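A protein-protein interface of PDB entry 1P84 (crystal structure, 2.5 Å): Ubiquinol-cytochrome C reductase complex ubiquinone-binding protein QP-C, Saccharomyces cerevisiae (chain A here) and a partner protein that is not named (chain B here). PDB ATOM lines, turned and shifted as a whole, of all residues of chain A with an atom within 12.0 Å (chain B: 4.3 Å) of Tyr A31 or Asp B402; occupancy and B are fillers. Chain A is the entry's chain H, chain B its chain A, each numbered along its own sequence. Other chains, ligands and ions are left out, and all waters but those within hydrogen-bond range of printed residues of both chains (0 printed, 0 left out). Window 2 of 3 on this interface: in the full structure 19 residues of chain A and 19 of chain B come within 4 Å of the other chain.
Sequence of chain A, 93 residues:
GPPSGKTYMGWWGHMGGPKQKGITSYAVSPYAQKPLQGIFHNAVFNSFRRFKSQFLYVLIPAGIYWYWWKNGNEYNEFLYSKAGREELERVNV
The side-chain carboxylate (OD2) of Asp B404 lies within hydrogen-bond range of the side-chain hydroxyl (OG) of Ser A29.
The side-chain carboxylate (OD1) of Asp B402 lies within salt-bridge range of the guanidinium group (NH1) of Arg B423, 2.7 Å away. O of Met B426 is in hydrogen-bond range of N of Asp B402 (2.9 Å). NE of Arg B423 is in hydrogen-bond range of O of Gln B403 (3.4 Å). The side-chain amide nitrogen (NE2) of Gln A33 lies within hydrogen-bond range of the backbone carbonyl oxygen (O) of Ser A29, 3.5 Å away. NH2 of Arg B423 lies within salt-bridge range of OD2 of Asp B404 (2.5 Å). N of Tyr A31 lies close to OG of Ser A29 (3.0 Å).
CG of Pro A30 touches SD of Met B420 (3.9 Å). OH of Tyr A31 touches OD1 of Asp B402, 3.8 Å away. CB of Tyr A31 touches OD2 of Asp B404, 3.4 Å away. Tyr A31 touches Arg B423 (CD1 to NH2, 3.0 Å).
Of the printed residues of chain B, Ser A29 touches Asp B404. Printed residues of chain B within 4 Å of Pro A30: Met B420. Of chain B, only Asp B402, Asp B404 and Arg B423 come within 4 Å of Tyr A31. No residue of chain A comes within 4 Å of Trp B401. Gln B403 touches none of the printed residues of chain A. Asp B404 touches just these residues of chain A: Ser A29 and Tyr A31. Of chain A, only Pro A30 comes within 4 Å of Met B420. The nearest residue of chain B that does not touch Tyr A31 is Met B420 (4.2 Å). The nearest printed residue of chain B that does not touch Pro A30 is Asp B404 (5.7 Å).
Of the 10 printed residues of chain A, 3 touch a printed residue of chain B. Hydrophobic or aromatic side chains of chain A that line the printed part of chain B: Pro A30 and Tyr A31. Of the 8 printed residues of chain B, 4 touch a printed residue of chain A. Hydrophobic or aromatic side chains of chain B within 4 Å of the printed part of chain A: Met B420. Among the printed residues, 5 pairs touch across the chains. Among the printed residues, no Asp or Glu carboxylate lies within 4 Å of a Lys or Arg side-chain nitrogen of the other chain.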
ATOM      1  N   ALA A  27      -4.251 -21.503  -0.121  1.00  0.00           N
ATOM      2  CA  ALA A  27      -4.588 -22.658  -0.939  1.00  0.00           C
ATOM      3  C   ALA A  27      -3.506 -22.921  -1.968  1.00  0.00           C
ATOM      4  O   ALA A  27      -2.738 -22.033  -2.315  1.00  0.00           O
ATOM      5  CB  ALA A  27      -5.944 -22.465  -1.620  1.00  0.00           C
ATOM      6  N   VAL A  28      -3.469 -24.153  -2.451  1.00  0.00           N
ATOM      7  CA  VAL A  28      -2.498 -24.586  -3.438  1.00  0.00           C
ATOM      8  C   VAL A  28      -3.237 -25.154  -4.643  1.00  0.00           C
ATOM      9  O   VAL A  28      -4.208 -25.900  -4.486  1.00  0.00           O
ATOM     10  CB  VAL A  28      -1.560 -25.664  -2.823  1.00  0.00           C
ATOM     11  CG1 VAL A  28      -0.844 -26.463  -3.907  1.00  0.00           C
ATOM     12  CG2 VAL A  28      -0.545 -24.991  -1.912  1.00  0.00           C
ATOM     13  N   SER A  29      -2.782 -24.795  -5.840  1.00  0.00           N
ATOM     14  CA  SER A  29      -3.402 -25.264  -7.071  1.00  0.00           C
ATOM     15  C   SER A  29      -3.527 -26.779  -7.138  1.00  0.00           C
ATOM     16  O   SER A  29      -2.623 -27.497  -6.716  1.00  0.00           O
ATOM     17  CB  SER A  29      -2.604 -24.794  -8.288  1.00  0.00           C
ATOM     18  OG  SER A  29      -3.062 -25.433  -9.476  1.00  0.00           O
ATOM     19  N   PRO A  30      -4.673 -27.282  -7.637  1.00  0.00           N
ATOM     20  CA  PRO A  30      -4.945 -28.713  -7.781  1.00  0.00           C
ATOM     21  C   PRO A  30      -3.930 -29.307  -8.742  1.00  0.00           C
ATOM     22  O   PRO A  30      -3.650 -30.502  -8.718  1.00  0.00           O
ATOM     23  CB  PRO A  30      -6.335 -28.724  -8.412  1.00  0.00           C
ATOM     24  CG  PRO A  30      -6.972 -27.532  -7.809  1.00  0.00           C
ATOM     25  CD  PRO A  30      -5.888 -26.496  -7.913  1.00  0.00           C
ATOM     26  N   TYR A  31      -3.395 -28.451  -9.603  1.00  0.00           N
ATOM     27  CA  TYR A  31      -2.408 -28.855 -10.595  1.00  0.00           C
ATOM     28  C   TYR A  31      -1.070 -29.225  -9.966  1.00  0.00           C
ATOM     29  O   TYR A  31      -0.365 -30.098 -10.466  1.00  0.00           O
ATOM     30  CB  TYR A  31      -2.210 -27.735 -11.610  1.00  0.00           C
ATOM     31  CG  TYR A  31      -3.286 -27.661 -12.669  1.00  0.00           C
ATOM     32  CD1 TYR A  31      -4.368 -26.785 -12.545  1.00  0.00           C
ATOM     33  CD2 TYR A  31      -3.188 -28.424 -13.832  1.00  0.00           C
ATOM     34  CE1 TYR A  31      -5.313 -26.664 -13.558  1.00  0.00           C
ATOM     35  CE2 TYR A  31      -4.127 -28.312 -14.849  1.00  0.00           C
ATOM     36  CZ  TYR A  31      -5.180 -27.432 -14.711  1.00  0.00           C
ATOM     37  OH  TYR A  31      -6.084 -27.309 -15.744  1.00  0.00           O
ATOM     38  N   ALA A  32      -0.740 -28.573  -8.855  1.00  0.00           N
ATOM     39  CA  ALA A  32       0.511 -28.822  -8.159  1.00  0.00           C
ATOM     40  C   ALA A  32       0.398 -29.899  -7.086  1.00  0.00           C
ATOM     41  O   ALA A  32       1.375 -30.193  -6.397  1.00  0.00           O
ATOM     42  CB  ALA A  32       1.022 -27.530  -7.546  1.00  0.00           C
ATOM     43  N   GLN A  33      -0.788 -30.479  -6.932  1.00  0.00           N
ATOM     44  CA  GLN A  33      -1.000 -31.512  -5.919  1.00  0.00           C
ATOM     45  C   GLN A  33      -0.800 -32.931  -6.430  1.00  0.00           C
ATOM     46  O   GLN A  33      -0.930 -33.215  -7.624  1.00  0.00           O
ATOM     47  CB  GLN A  33      -2.372 -31.357  -5.257  1.00  0.00           C
ATOM     48  CG  GLN A  33      -2.476 -30.104  -4.408  1.00  0.00           C
ATOM     49  CD  GLN A  33      -3.853 -29.887  -3.812  1.00  0.00           C
ATOM     50  OE1 GLN A  33      -4.443 -30.793  -3.222  1.00  0.00           O
ATOM     51  NE2 GLN A  33      -4.362 -28.670  -3.942  1.00  0.00           N
ATOM     52  N   LYS A  34      -0.452 -33.809  -5.499  1.00  0.00           N
ATOM     53  CA  LYS A  34      -0.196 -35.211  -5.782  1.00  0.00           C
ATOM     54  C   LYS A  34      -1.406 -35.836  -6.457  1.00  0.00           C
ATOM     55  O   LYS A  34      -2.521 -35.756  -5.937  1.00  0.00           O
ATOM     56  CB  LYS A  34       0.112 -35.933  -4.468  1.00  0.00           C
ATOM     57  CG  LYS A  34       0.979 -37.179  -4.591  1.00  0.00           C
ATOM     58  CD  LYS A  34       2.010 -37.217  -3.463  1.00  0.00           C
ATOM     59  CE  LYS A  34       1.356 -37.028  -2.094  1.00  0.00           C
ATOM     60  NZ  LYS A  34       2.356 -36.903  -0.997  1.00  0.00           N
ATOM     61  N   PRO A  35      -1.206 -36.443  -7.642  1.00  0.00           N
ATOM     62  CA  PRO A  35      -2.303 -37.080  -8.377  1.00  0.00           C
ATOM     63  C   PRO A  35      -3.062 -38.036  -7.463  1.00  0.00           C
ATOM     64  O   PRO A  35      -2.464 -38.743  -6.647  1.00  0.00           O
ATOM     65  CB  PRO A  35      -1.579 -37.814  -9.514  1.00  0.00           C
ATOM     66  CG  PRO A  35      -0.192 -38.032  -8.974  1.00  0.00           C
ATOM     67  CD  PRO A  35       0.083 -36.716  -8.298  1.00  0.00           C
ATOM     68  N   LEU A  36      -4.383 -38.011  -7.576  1.00  0.00           N
ATOM     69  CA  LEU A  36      -5.265 -38.833  -6.755  1.00  0.00           C
ATOM     70  C   LEU A  36      -4.841 -40.297  -6.595  1.00  0.00           C
ATOM     71  O   LEU A  36      -5.068 -41.130  -7.476  1.00  0.00           O
ATOM     72  CB  LEU A  36      -6.692 -38.735  -7.295  1.00  0.00           C
ATOM     73  CG  LEU A  36      -7.134 -37.290  -7.559  1.00  0.00           C
ATOM     74  CD1 LEU A  36      -8.442 -37.299  -8.303  1.00  0.00           C
ATOM     75  CD2 LEU A  36      -7.238 -36.496  -6.254  1.00  0.00           C
ATOM     76  N   LEU B 400       2.127 -18.193 -20.238  1.00  0.00           N
ATOM     77  CA  LEU B 400       0.758 -17.799 -19.923  1.00  0.00           C
ATOM     78  C   LEU B 400      -0.357 -18.797 -20.215  1.00  0.00           C
ATOM     79  O   LEU B 400      -1.249 -18.967 -19.389  1.00  0.00           O
ATOM     80  CB  LEU B 400       0.443 -16.468 -20.598  1.00  0.00           C
ATOM     81  CG  LEU B 400       0.720 -15.173 -19.830  1.00  0.00           C
ATOM     82  CD1 LEU B 400       2.084 -15.195 -19.198  1.00  0.00           C
ATOM     83  CD2 LEU B 400       0.603 -13.989 -20.769  1.00  0.00           C
ATOM     84  N   TRP B 401      -0.291 -19.485 -21.354  1.00  0.00           N
ATOM     85  CA  TRP B 401      -1.339 -20.433 -21.737  1.00  0.00           C
ATOM     86  C   TRP B 401      -1.472 -21.698 -20.887  1.00  0.00           C
ATOM     87  O   TRP B 401      -0.603 -22.574 -20.912  1.00  0.00           O
ATOM     88  CB  TRP B 401      -1.207 -20.813 -23.214  1.00  0.00           C
ATOM     89  CG  TRP B 401      -2.437 -21.483 -23.797  1.00  0.00           C
ATOM     90  CD1 TRP B 401      -2.665 -22.830 -23.919  1.00  0.00           C
ATOM     91  CD2 TRP B 401      -3.571 -20.831 -24.390  1.00  0.00           C
ATOM     92  NE1 TRP B 401      -3.865 -23.053 -24.562  1.00  0.00           N
ATOM     93  CE2 TRP B 401      -4.439 -21.843 -24.861  1.00  0.00           C
ATOM     94  CE3 TRP B 401      -3.935 -19.490 -24.574  1.00  0.00           C
ATOM     95  CZ2 TRP B 401      -5.644 -21.555 -25.506  1.00  0.00           C
ATOM     96  CZ3 TRP B 401      -5.134 -19.204 -25.214  1.00  0.00           C
ATOM     97  CH2 TRP B 401      -5.975 -20.237 -25.674  1.00  0.00           C
ATOM     98  N   ASP B 402      -2.594 -21.792 -20.168  1.00  0.00           N
ATOM     99  CA  ASP B 402      -2.901 -22.935 -19.312  1.00  0.00           C
ATOM    100  C   ASP B 402      -1.781 -23.222 -18.312  1.00  0.00           C
ATOM    101  O   ASP B 402      -1.318 -24.357 -18.178  1.00  0.00           O
ATOM    102  CB  ASP B 402      -3.193 -24.163 -20.188  1.00  0.00           C
ATOM    103  CG  ASP B 402      -3.882 -25.287 -19.437  1.00  0.00           C
ATOM    104  OD1 ASP B 402      -4.395 -25.086 -18.323  1.00  0.00           O
ATOM    105  OD2 ASP B 402      -3.923 -26.403 -19.980  1.00  0.00           O
ATOM    106  N   GLN B 403      -1.364 -22.179 -17.601  1.00  0.00           N
ATOM    107  CA  GLN B 403      -0.307 -22.279 -16.600  1.00  0.00           C
ATOM    108  C   GLN B 403      -0.813 -21.835 -15.227  1.00  0.00           C
ATOM    109  O   GLN B 403      -1.665 -20.940 -15.131  1.00  0.00           O
ATOM    110  CB  GLN B 403       0.885 -21.399 -16.999  1.00  0.00           C
ATOM    111  CG  GLN B 403       1.664 -21.883 -18.203  1.00  0.00           C
ATOM    112  CD  GLN B 403       2.334 -23.217 -17.958  1.00  0.00           C
ATOM    113  OE1 GLN B 403       2.897 -23.454 -16.887  1.00  0.00           O
ATOM    114  NE2 GLN B 403       2.277 -24.101 -18.951  1.00  0.00           N
ATOM    115  N   ASP B 404      -0.258 -22.425 -14.166  1.00  0.00           N
ATOM    116  CA  ASP B 404      -0.655 -22.073 -12.810  1.00  0.00           C
ATOM    117  C   ASP B 404      -0.400 -20.608 -12.564  1.00  0.00           C
ATOM    118  O   ASP B 404       0.412 -20.005 -13.239  1.00  0.00           O
ATOM    119  CB  ASP B 404       0.124 -22.889 -11.783  1.00  0.00           C
ATOM    120  CG  ASP B 404      -0.492 -24.252 -11.521  1.00  0.00           C
ATOM    121  OD1 ASP B 404       0.272 -25.230 -11.334  1.00  0.00           O
ATOM    122  OD2 ASP B 404      -1.735 -24.343 -11.471  1.00  0.00           O
ATOM    123  N   MET B 420      -9.781 -22.061  -8.981  1.00  0.00           N
ATOM    124  CA  MET B 420     -10.083 -22.748 -10.233  1.00  0.00           C
ATOM    125  C   MET B 420     -10.836 -21.931 -11.285  1.00  0.00           C
ATOM    126  O   MET B 420     -10.726 -22.213 -12.489  1.00  0.00           O
ATOM    127  CB  MET B 420     -10.794 -24.062  -9.968  1.00  0.00           C
ATOM    128  CG  MET B 420      -9.847 -25.120  -9.479  1.00  0.00           C
ATOM    129  SD  MET B 420      -8.477 -25.321 -10.633  1.00  0.00           S
ATOM    130  CE  MET B 420      -8.876 -26.943 -11.324  1.00  0.00           C
ATOM    131  N   ARG B 423      -8.045 -19.641 -12.519  1.00  0.00           N
ATOM    132  CA  ARG B 423      -7.134 -20.553 -13.206  1.00  0.00           C
ATOM    133  C   ARG B 423      -7.644 -21.014 -14.575  1.00  0.00           C
ATOM    134  O   ARG B 423      -6.874 -21.107 -15.531  1.00  0.00           O
ATOM    135  CB  ARG B 423      -6.813 -21.745 -12.292  1.00  0.00           C
ATOM    136  CG  ARG B 423      -5.953 -22.842 -12.904  1.00  0.00           C
ATOM    137  CD  ARG B 423      -4.601 -22.344 -13.379  1.00  0.00           C
ATOM    138  NE  ARG B 423      -4.283 -22.991 -14.652  1.00  0.00           N
ATOM    139  CZ  ARG B 423      -3.456 -24.019 -14.781  1.00  0.00           C
ATOM    140  NH1 ARG B 423      -3.242 -24.566 -15.966  1.00  0.00           N
ATOM    141  NH2 ARG B 423      -2.797 -24.472 -13.731  1.00  0.00           N
ATOM    142  N   MET B 426      -7.024 -18.946 -17.938  1.00  0.00           N
ATOM    143  CA  MET B 426      -5.701 -18.855 -18.535  1.00  0.00           C
ATOM    144  C   MET B 426      -5.697 -19.524 -19.899  1.00  0.00           C
ATOM    145  O   MET B 426      -4.634 -19.809 -20.459  1.00  0.00           O
ATOM    146  CB  MET B 426      -4.647 -19.498 -17.633  1.00  0.00           C
ATOM    147  CG  MET B 426      -4.478 -18.810 -16.301  1.00  0.00           C
ATOM    148  SD  MET B 426      -4.149 -17.052 -16.483  1.00  0.00           S
ATOM    149  CE  MET B 426      -2.414 -17.085 -16.803  1.00  0.00           C
